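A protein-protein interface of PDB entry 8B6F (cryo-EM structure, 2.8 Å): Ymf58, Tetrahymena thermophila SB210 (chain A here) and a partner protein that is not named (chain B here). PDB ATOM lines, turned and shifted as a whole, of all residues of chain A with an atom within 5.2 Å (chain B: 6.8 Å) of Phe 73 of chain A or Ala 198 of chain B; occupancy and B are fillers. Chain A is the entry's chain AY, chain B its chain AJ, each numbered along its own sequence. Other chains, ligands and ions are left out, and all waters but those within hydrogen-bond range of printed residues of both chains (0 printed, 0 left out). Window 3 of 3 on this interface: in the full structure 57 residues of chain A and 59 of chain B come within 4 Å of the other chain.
The backbone carbonyl oxygen (O) of Gly 195 of chain B lies within hydrogen-bond range of the side-chain sulfur (SG) of Cys 199 of chain B (3.2 Å).
Among the printed residues, pairs that only touch across the chains: Leu 76 of chain A with Cys 199 of chain B (3.3 Å), Leu 76 of chain A with Leu 202 of chain B (3.4 Å), Leu 69 of chain A with Leu 191 of chain B (3.6 Å), Phe 73 of chain A with Cys 199 of chain B (3.8 Å), Leu 69 of chain A with Gly 195 of chain B (3.8 Å) and Phe 73 of chain A with Ala 198 of chain B (3.9 Å).
Of the printed residues of chain A, Leu 191 of chain B touches Leu 69 (3.6 Å).
Leu 194 of chain B touches none of the printed residues of chain A.
Of the printed residues of chain A, Gly 195 of chain B touches Leu 69 (3.8 Å).
Of chain A, only Phe 73 comes within 4 Å of Ala 198 of chain B.
Of the printed residues of chain A, Cys 199 of chain B touches Phe 73 (3.8 Å) and Leu 76 (3.3 Å).
The nearest residue of chain B that does not touch Phe 73 of chain A is Gly 195 of chain B (4.1 Å).
The nearest printed residue of chain A that does not touch Ala 198 of chain B is Leu 76 of chain A (5.2 Å).
The nearest printed residue of chain A that does not touch Leu 191 of chain B is Phe 73 of chain A (6.4 Å).
Of the 12 printed residues of chain B, 5 touch a printed residue of chain A.
Printed residues of chain B that touch a printed residue of chain A: Leu 191, Gly 195, Ala 198, Cys 199 and Leu 202.
Hydrophobic or aromatic side chains of chain B within 4 Å of the printed part of chain A: Leu 191, Ala 198 and Leu 202.
Of the 11 printed residues of chain A, 3 touch a printed residue of chain B.
Hydrophobic or aromatic side chains of chain A that line the printed part of chain B: Leu 69, Phe 73 and Leu 76.
Among the printed residues, 6 pairs touch across the chains.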
ATOM      1  N   GLY A  68     -26.555  -6.598   9.737  1.00  0.00           N
ATOM      2  CA  GLY A  68     -26.681  -6.663   8.290  1.00  0.00           C
ATOM      3  C   GLY A  68     -26.369  -8.040   7.740  1.00  0.00           C
ATOM      4  O   GLY A  68     -27.087  -8.551   6.878  1.00  0.00           O
ATOM      5  N   LEU A  69     -25.294  -8.661   8.228  1.00  0.00           N
ATOM      6  CA  LEU A  69     -24.950 -10.002   7.766  1.00  0.00           C
ATOM      7  C   LEU A  69     -26.039 -11.003   8.126  1.00  0.00           C
ATOM      8  O   LEU A  69     -26.412 -11.848   7.305  1.00  0.00           O
ATOM      9  CB  LEU A  69     -23.608 -10.431   8.355  1.00  0.00           C
ATOM     10  CG  LEU A  69     -23.116 -11.822   7.949  1.00  0.00           C
ATOM     11  CD1 LEU A  69     -22.945 -11.931   6.441  1.00  0.00           C
ATOM     12  CD2 LEU A  69     -21.815 -12.146   8.659  1.00  0.00           C
ATOM     13  N   GLU A  70     -26.559 -10.926   9.352  1.00  0.00           N
ATOM     14  CA  GLU A  70     -27.621 -11.840   9.760  1.00  0.00           C
ATOM     15  C   GLU A  70     -28.882 -11.612   8.940  1.00  0.00           C
ATOM     16  O   GLU A  70     -29.596 -12.563   8.606  1.00  0.00           O
ATOM     17  CB  GLU A  70     -27.911 -11.686  11.252  1.00  0.00           C
ATOM     18  CG  GLU A  70     -26.808 -12.232  12.142  1.00  0.00           C
ATOM     19  CD  GLU A  70     -27.226 -12.334  13.595  1.00  0.00           C
ATOM     20  OE1 GLU A  70     -28.392 -12.007  13.904  1.00  0.00           O
ATOM     21  OE2 GLU A  70     -26.392 -12.745  14.429  1.00  0.00           O
ATOM     22  N   PHE A  71     -29.171 -10.354   8.601  1.00  0.00           N
ATOM     23  CA  PHE A  71     -30.338 -10.064   7.777  1.00  0.00           C
ATOM     24  C   PHE A  71     -30.166 -10.631   6.374  1.00  0.00           C
ATOM     25  O   PHE A  71     -31.125 -11.143   5.785  1.00  0.00           O
ATOM     26  CB  PHE A  71     -30.584  -8.556   7.723  1.00  0.00           C
ATOM     27  CG  PHE A  71     -32.007  -8.188   7.411  1.00  0.00           C
ATOM     28  CD1 PHE A  71     -32.951  -8.114   8.421  1.00  0.00           C
ATOM     29  CD2 PHE A  71     -32.399  -7.911   6.112  1.00  0.00           C
ATOM     30  CE1 PHE A  71     -34.262  -7.775   8.143  1.00  0.00           C
ATOM     31  CE2 PHE A  71     -33.708  -7.571   5.826  1.00  0.00           C
ATOM     32  CZ  PHE A  71     -34.640  -7.502   6.843  1.00  0.00           C
ATOM     33  N   SER A  72     -28.954 -10.554   5.824  1.00  0.00           N
ATOM     34  CA  SER A  72     -28.696 -11.168   4.527  1.00  0.00           C
ATOM     35  C   SER A  72     -28.932 -12.671   4.581  1.00  0.00           C
ATOM     36  O   SER A  72     -29.564 -13.245   3.689  1.00  0.00           O
ATOM     37  CB  SER A  72     -27.262 -10.870   4.090  1.00  0.00           C
ATOM     38  OG  SER A  72     -27.050  -9.478   3.937  1.00  0.00           O
ATOM     39  N   PHE A  73     -28.415 -13.330   5.621  1.00  0.00           N
ATOM     40  CA  PHE A  73     -28.638 -14.763   5.769  1.00  0.00           C
ATOM     41  C   PHE A  73     -30.121 -15.073   5.913  1.00  0.00           C
ATOM     42  O   PHE A  73     -30.615 -16.058   5.351  1.00  0.00           O
ATOM     43  CB  PHE A  73     -27.859 -15.296   6.972  1.00  0.00           C
ATOM     44  CG  PHE A  73     -26.386 -15.451   6.724  1.00  0.00           C
ATOM     45  CD1 PHE A  73     -25.920 -16.043   5.560  1.00  0.00           C
ATOM     46  CD2 PHE A  73     -25.466 -15.006   7.655  1.00  0.00           C
ATOM     47  CE1 PHE A  73     -24.569 -16.188   5.332  1.00  0.00           C
ATOM     48  CE2 PHE A  73     -24.110 -15.147   7.433  1.00  0.00           C
ATOM     49  CZ  PHE A  73     -23.662 -15.739   6.269  1.00  0.00           C
ATOM     50  N   GLY A  74     -30.847 -14.241   6.657  1.00  0.00           N
ATOM     51  CA  GLY A  74     -32.274 -14.459   6.816  1.00  0.00           C
ATOM     52  C   GLY A  74     -33.036 -14.325   5.513  1.00  0.00           C
ATOM     53  O   GLY A  74     -33.946 -15.109   5.232  1.00  0.00           O
ATOM     54  N   ILE A  75     -32.679 -13.334   4.697  1.00  0.00           N
ATOM     55  CA  ILE A  75     -33.308 -13.198   3.388  1.00  0.00           C
ATOM     56  C   ILE A  75     -33.068 -14.451   2.559  1.00  0.00           C
ATOM     57  O   ILE A  75     -33.982 -14.977   1.912  1.00  0.00           O
ATOM     58  CB  ILE A  75     -32.782 -11.942   2.672  1.00  0.00           C
ATOM     59  CG1 ILE A  75     -33.290 -10.682   3.373  1.00  0.00           C
ATOM     60  CG2 ILE A  75     -33.193 -11.943   1.198  1.00  0.00           C
ATOM     61  CD1 ILE A  75     -32.667  -9.402   2.862  1.00  0.00           C
ATOM     62  N   LEU A  76     -31.830 -14.944   2.557  1.00  0.00           N
ATOM     63  CA  LEU A  76     -31.513 -16.128   1.769  1.00  0.00           C
ATOM     64  C   LEU A  76     -32.303 -17.340   2.245  1.00  0.00           C
ATOM     65  O   LEU A  76     -32.810 -18.118   1.430  1.00  0.00           O
ATOM     66  CB  LEU A  76     -30.013 -16.402   1.826  1.00  0.00           C
ATOM     67  CG  LEU A  76     -29.123 -15.386   1.103  1.00  0.00           C
ATOM     68  CD1 LEU A  76     -27.662 -15.711   1.321  1.00  0.00           C
ATOM     69  CD2 LEU A  76     -29.431 -15.341  -0.383  1.00  0.00           C
ATOM     70  N   ILE A  77     -32.416 -17.522   3.561  1.00  0.00           N
ATOM     71  CA  ILE A  77     -33.162 -18.664   4.080  1.00  0.00           C
ATOM     72  C   ILE A  77     -34.641 -18.531   3.743  1.00  0.00           C
ATOM     73  O   ILE A  77     -35.297 -19.511   3.374  1.00  0.00           O
ATOM     74  CB  ILE A  77     -32.936 -18.813   5.596  1.00  0.00           C
ATOM     75  CG1 ILE A  77     -31.459 -19.087   5.890  1.00  0.00           C
ATOM     76  CG2 ILE A  77     -33.794 -19.943   6.160  1.00  0.00           C
ATOM     77  CD1 ILE A  77     -31.094 -18.986   7.356  1.00  0.00           C
ATOM     78  N   ALA A  78     -35.194 -17.322   3.870  1.00  0.00           N
ATOM     79  CA  ALA A  78     -36.602 -17.121   3.541  1.00  0.00           C
ATOM     80  C   ALA A  78     -36.881 -17.433   2.077  1.00  0.00           C
ATOM     81  O   ALA A  78     -37.945 -17.960   1.738  1.00  0.00           O
ATOM     82  CB  ALA A  78     -37.015 -15.687   3.868  1.00  0.00           C
ATOM     83  N   LEU B 191     -15.092 -11.311   8.360  1.00  0.00           N
ATOM     84  CA  LEU B 191     -16.420 -11.884   8.541  1.00  0.00           C
ATOM     85  C   LEU B 191     -17.335 -11.538   7.376  1.00  0.00           C
ATOM     86  O   LEU B 191     -18.086 -12.391   6.891  1.00  0.00           O
ATOM     87  CB  LEU B 191     -17.014 -11.388   9.860  1.00  0.00           C
ATOM     88  CG  LEU B 191     -18.485 -11.698  10.136  1.00  0.00           C
ATOM     89  CD1 LEU B 191     -18.703 -13.189  10.237  1.00  0.00           C
ATOM     90  CD2 LEU B 191     -18.944 -11.007  11.407  1.00  0.00           C
ATOM     91  N   LEU B 193     -16.399 -10.743   4.282  1.00  0.00           N
ATOM     92  CA  LEU B 193     -15.937 -11.473   3.104  1.00  0.00           C
ATOM     93  C   LEU B 193     -16.414 -12.918   3.142  1.00  0.00           C
ATOM     94  O   LEU B 193     -16.956 -13.434   2.159  1.00  0.00           O
ATOM     95  CB  LEU B 193     -14.413 -11.414   3.016  1.00  0.00           C
ATOM     96  CG  LEU B 193     -13.782 -12.209   1.870  1.00  0.00           C
ATOM     97  CD1 LEU B 193     -14.229 -11.678   0.520  1.00  0.00           C
ATOM     98  CD2 LEU B 193     -12.275 -12.175   1.983  1.00  0.00           C
ATOM     99  N   LEU B 194     -16.210 -13.591   4.275  1.00  0.00           N
ATOM    100  CA  LEU B 194     -16.648 -14.974   4.404  1.00  0.00           C
ATOM    101  C   LEU B 194     -18.162 -15.083   4.291  1.00  0.00           C
ATOM    102  O   LEU B 194     -18.678 -16.073   3.764  1.00  0.00           O
ATOM    103  CB  LEU B 194     -16.164 -15.559   5.729  1.00  0.00           C
ATOM    104  CG  LEU B 194     -16.251 -17.080   5.867  1.00  0.00           C
ATOM    105  CD1 LEU B 194     -15.370 -17.787   4.850  1.00  0.00           C
ATOM    106  CD2 LEU B 194     -15.869 -17.491   7.273  1.00  0.00           C
ATOM    107  N   GLY B 195     -18.885 -14.077   4.785  1.00  0.00           N
ATOM    108  CA  GLY B 195     -20.331 -14.079   4.653  1.00  0.00           C
ATOM    109  C   GLY B 195     -20.786 -13.935   3.215  1.00  0.00           C
ATOM    110  O   GLY B 195     -21.763 -14.562   2.799  1.00  0.00           O
ATOM    111  N   SER B 196     -20.089 -13.110   2.432  1.00  0.00           N
ATOM    112  CA  SER B 196     -20.393 -13.029   1.009  1.00  0.00           C
ATOM    113  C   SER B 196     -20.176 -14.376   0.332  1.00  0.00           C
ATOM    114  O   SER B 196     -21.001 -14.811  -0.481  1.00  0.00           O
ATOM    115  CB  SER B 196     -19.527 -11.958   0.347  1.00  0.00           C
ATOM    116  OG  SER B 196     -19.742 -10.690   0.940  1.00  0.00           O
ATOM    117  N   VAL B 197     -19.076 -15.054   0.656  1.00  0.00           N
ATOM    118  CA  VAL B 197     -18.827 -16.374   0.084  1.00  0.00           C
ATOM    119  C   VAL B 197     -19.944 -17.331   0.476  1.00  0.00           C
ATOM    120  O   VAL B 197     -20.446 -18.098  -0.355  1.00  0.00           O
ATOM    121  CB  VAL B 197     -17.447 -16.897   0.527  1.00  0.00           C
ATOM    122  CG1 VAL B 197     -17.224 -18.323   0.040  1.00  0.00           C
ATOM    123  CG2 VAL B 197     -16.345 -15.983   0.018  1.00  0.00           C
ATOM    124  N   ALA B 198     -20.347 -17.307   1.746  1.00  0.00           N
ATOM    125  CA  ALA B 198     -21.407 -18.197   2.206  1.00  0.00           C
ATOM    126  C   ALA B 198     -22.725 -17.890   1.510  1.00  0.00           C
ATOM    127  O   ALA B 198     -23.483 -18.804   1.167  1.00  0.00           O
ATOM    128  CB  ALA B 198     -21.567 -18.085   3.721  1.00  0.00           C
ATOM    129  N   CYS B 199     -23.021 -16.607   1.298  1.00  0.00           N
ATOM    130  CA  CYS B 199     -24.243 -16.241   0.592  1.00  0.00           C
ATOM    131  C   CYS B 199     -24.232 -16.760  -0.840  1.00  0.00           C
ATOM    132  O   CYS B 199     -25.244 -17.274  -1.328  1.00  0.00           O
ATOM    133  CB  CYS B 199     -24.419 -14.724   0.606  1.00  0.00           C
ATOM    134  SG  CYS B 199     -24.903 -14.046   2.209  1.00  0.00           S
ATOM    135  N   VAL B 200     -23.096 -16.635  -1.529  1.00  0.00           N
ATOM    136  CA  VAL B 200     -22.997 -17.155  -2.890  1.00  0.00           C
ATOM    137  C   VAL B 200     -23.211 -18.662  -2.902  1.00  0.00           C
ATOM    138  O   VAL B 200     -23.927 -19.195  -3.756  1.00  0.00           O
ATOM    139  CB  VAL B 200     -21.641 -16.769  -3.506  1.00  0.00           C
ATOM    140  CG1 VAL B 200     -21.429 -17.471  -4.840  1.00  0.00           C
ATOM    141  CG2 VAL B 200     -21.551 -15.266  -3.680  1.00  0.00           C
ATOM    142  N   ASN B 201     -22.590 -19.372  -1.961  1.00  0.00           N
ATOM    143  CA  ASN B 201     -22.742 -20.823  -1.914  1.00  0.00           C
ATOM    144  C   ASN B 201     -24.178 -21.220  -1.597  1.00  0.00           C
ATOM    145  O   ASN B 201     -24.685 -22.212  -2.133  1.00  0.00           O
ATOM    146  CB  ASN B 201     -21.774 -21.412  -0.894  1.00  0.00           C
ATOM    147  CG  ASN B 201     -20.345 -21.409  -1.392  1.00  0.00           C
ATOM    148  OD1 ASN B 201     -19.881 -22.380  -1.983  1.00  0.00           O
ATOM    149  ND2 ASN B 201     -19.643 -20.306  -1.166  1.00  0.00           N
ATOM    150  N   LEU B 202     -24.845 -20.468  -0.721  1.00  0.00           N
ATOM    151  CA  LEU B 202     -26.246 -20.749  -0.426  1.00  0.00           C
ATOM    152  C   LEU B 202     -27.118 -20.523  -1.653  1.00  0.00           C
ATOM    153  O   LEU B 202     -28.063 -21.281  -1.900  1.00  0.00           O
ATOM    154  CB  LEU B 202     -26.720 -19.891   0.747  1.00  0.00           C
ATOM    155  CG  LEU B 202     -28.171 -20.085   1.200  1.00  0.00           C
ATOM    156  CD1 LEU B 202     -28.507 -21.551   1.415  1.00  0.00           C
ATOM    157  CD2 LEU B 202     -28.407 -19.311   2.478  1.00  0.00           C
ATOM    158  N   TYR B 203     -26.821 -19.482  -2.430  1.00  0.00           N
ATOM    159  CA  TYR B 203     -27.542 -19.262  -3.679  1.00  0.00           C
ATOM    160  C   TYR B 203     -27.361 -20.438  -4.632  1.00  0.00           C
ATOM    161  O   TYR B 203     -28.325 -20.897  -5.254  1.00  0.00           O
ATOM    162  CB  TYR B 203     -27.063 -17.965  -4.326  1.00  0.00           C
ATOM    163  CG  TYR B 203     -27.605 -17.726  -5.714  1.00  0.00           C
ATOM    164  CD1 TYR B 203     -28.843 -17.129  -5.904  1.00  0.00           C
ATOM    165  CD2 TYR B 203     -26.871 -18.084  -6.835  1.00  0.00           C
ATOM    166  CE1 TYR B 203     -29.339 -16.904  -7.170  1.00  0.00           C
ATOM    167  CE2 TYR B 203     -27.355 -17.864  -8.105  1.00  0.00           C
ATOM    168  CZ  TYR B 203     -28.590 -17.275  -8.267  1.00  0.00           C
ATOM    169  OH  TYR B 203     -29.077 -17.053  -9.532  1.00  0.00           O
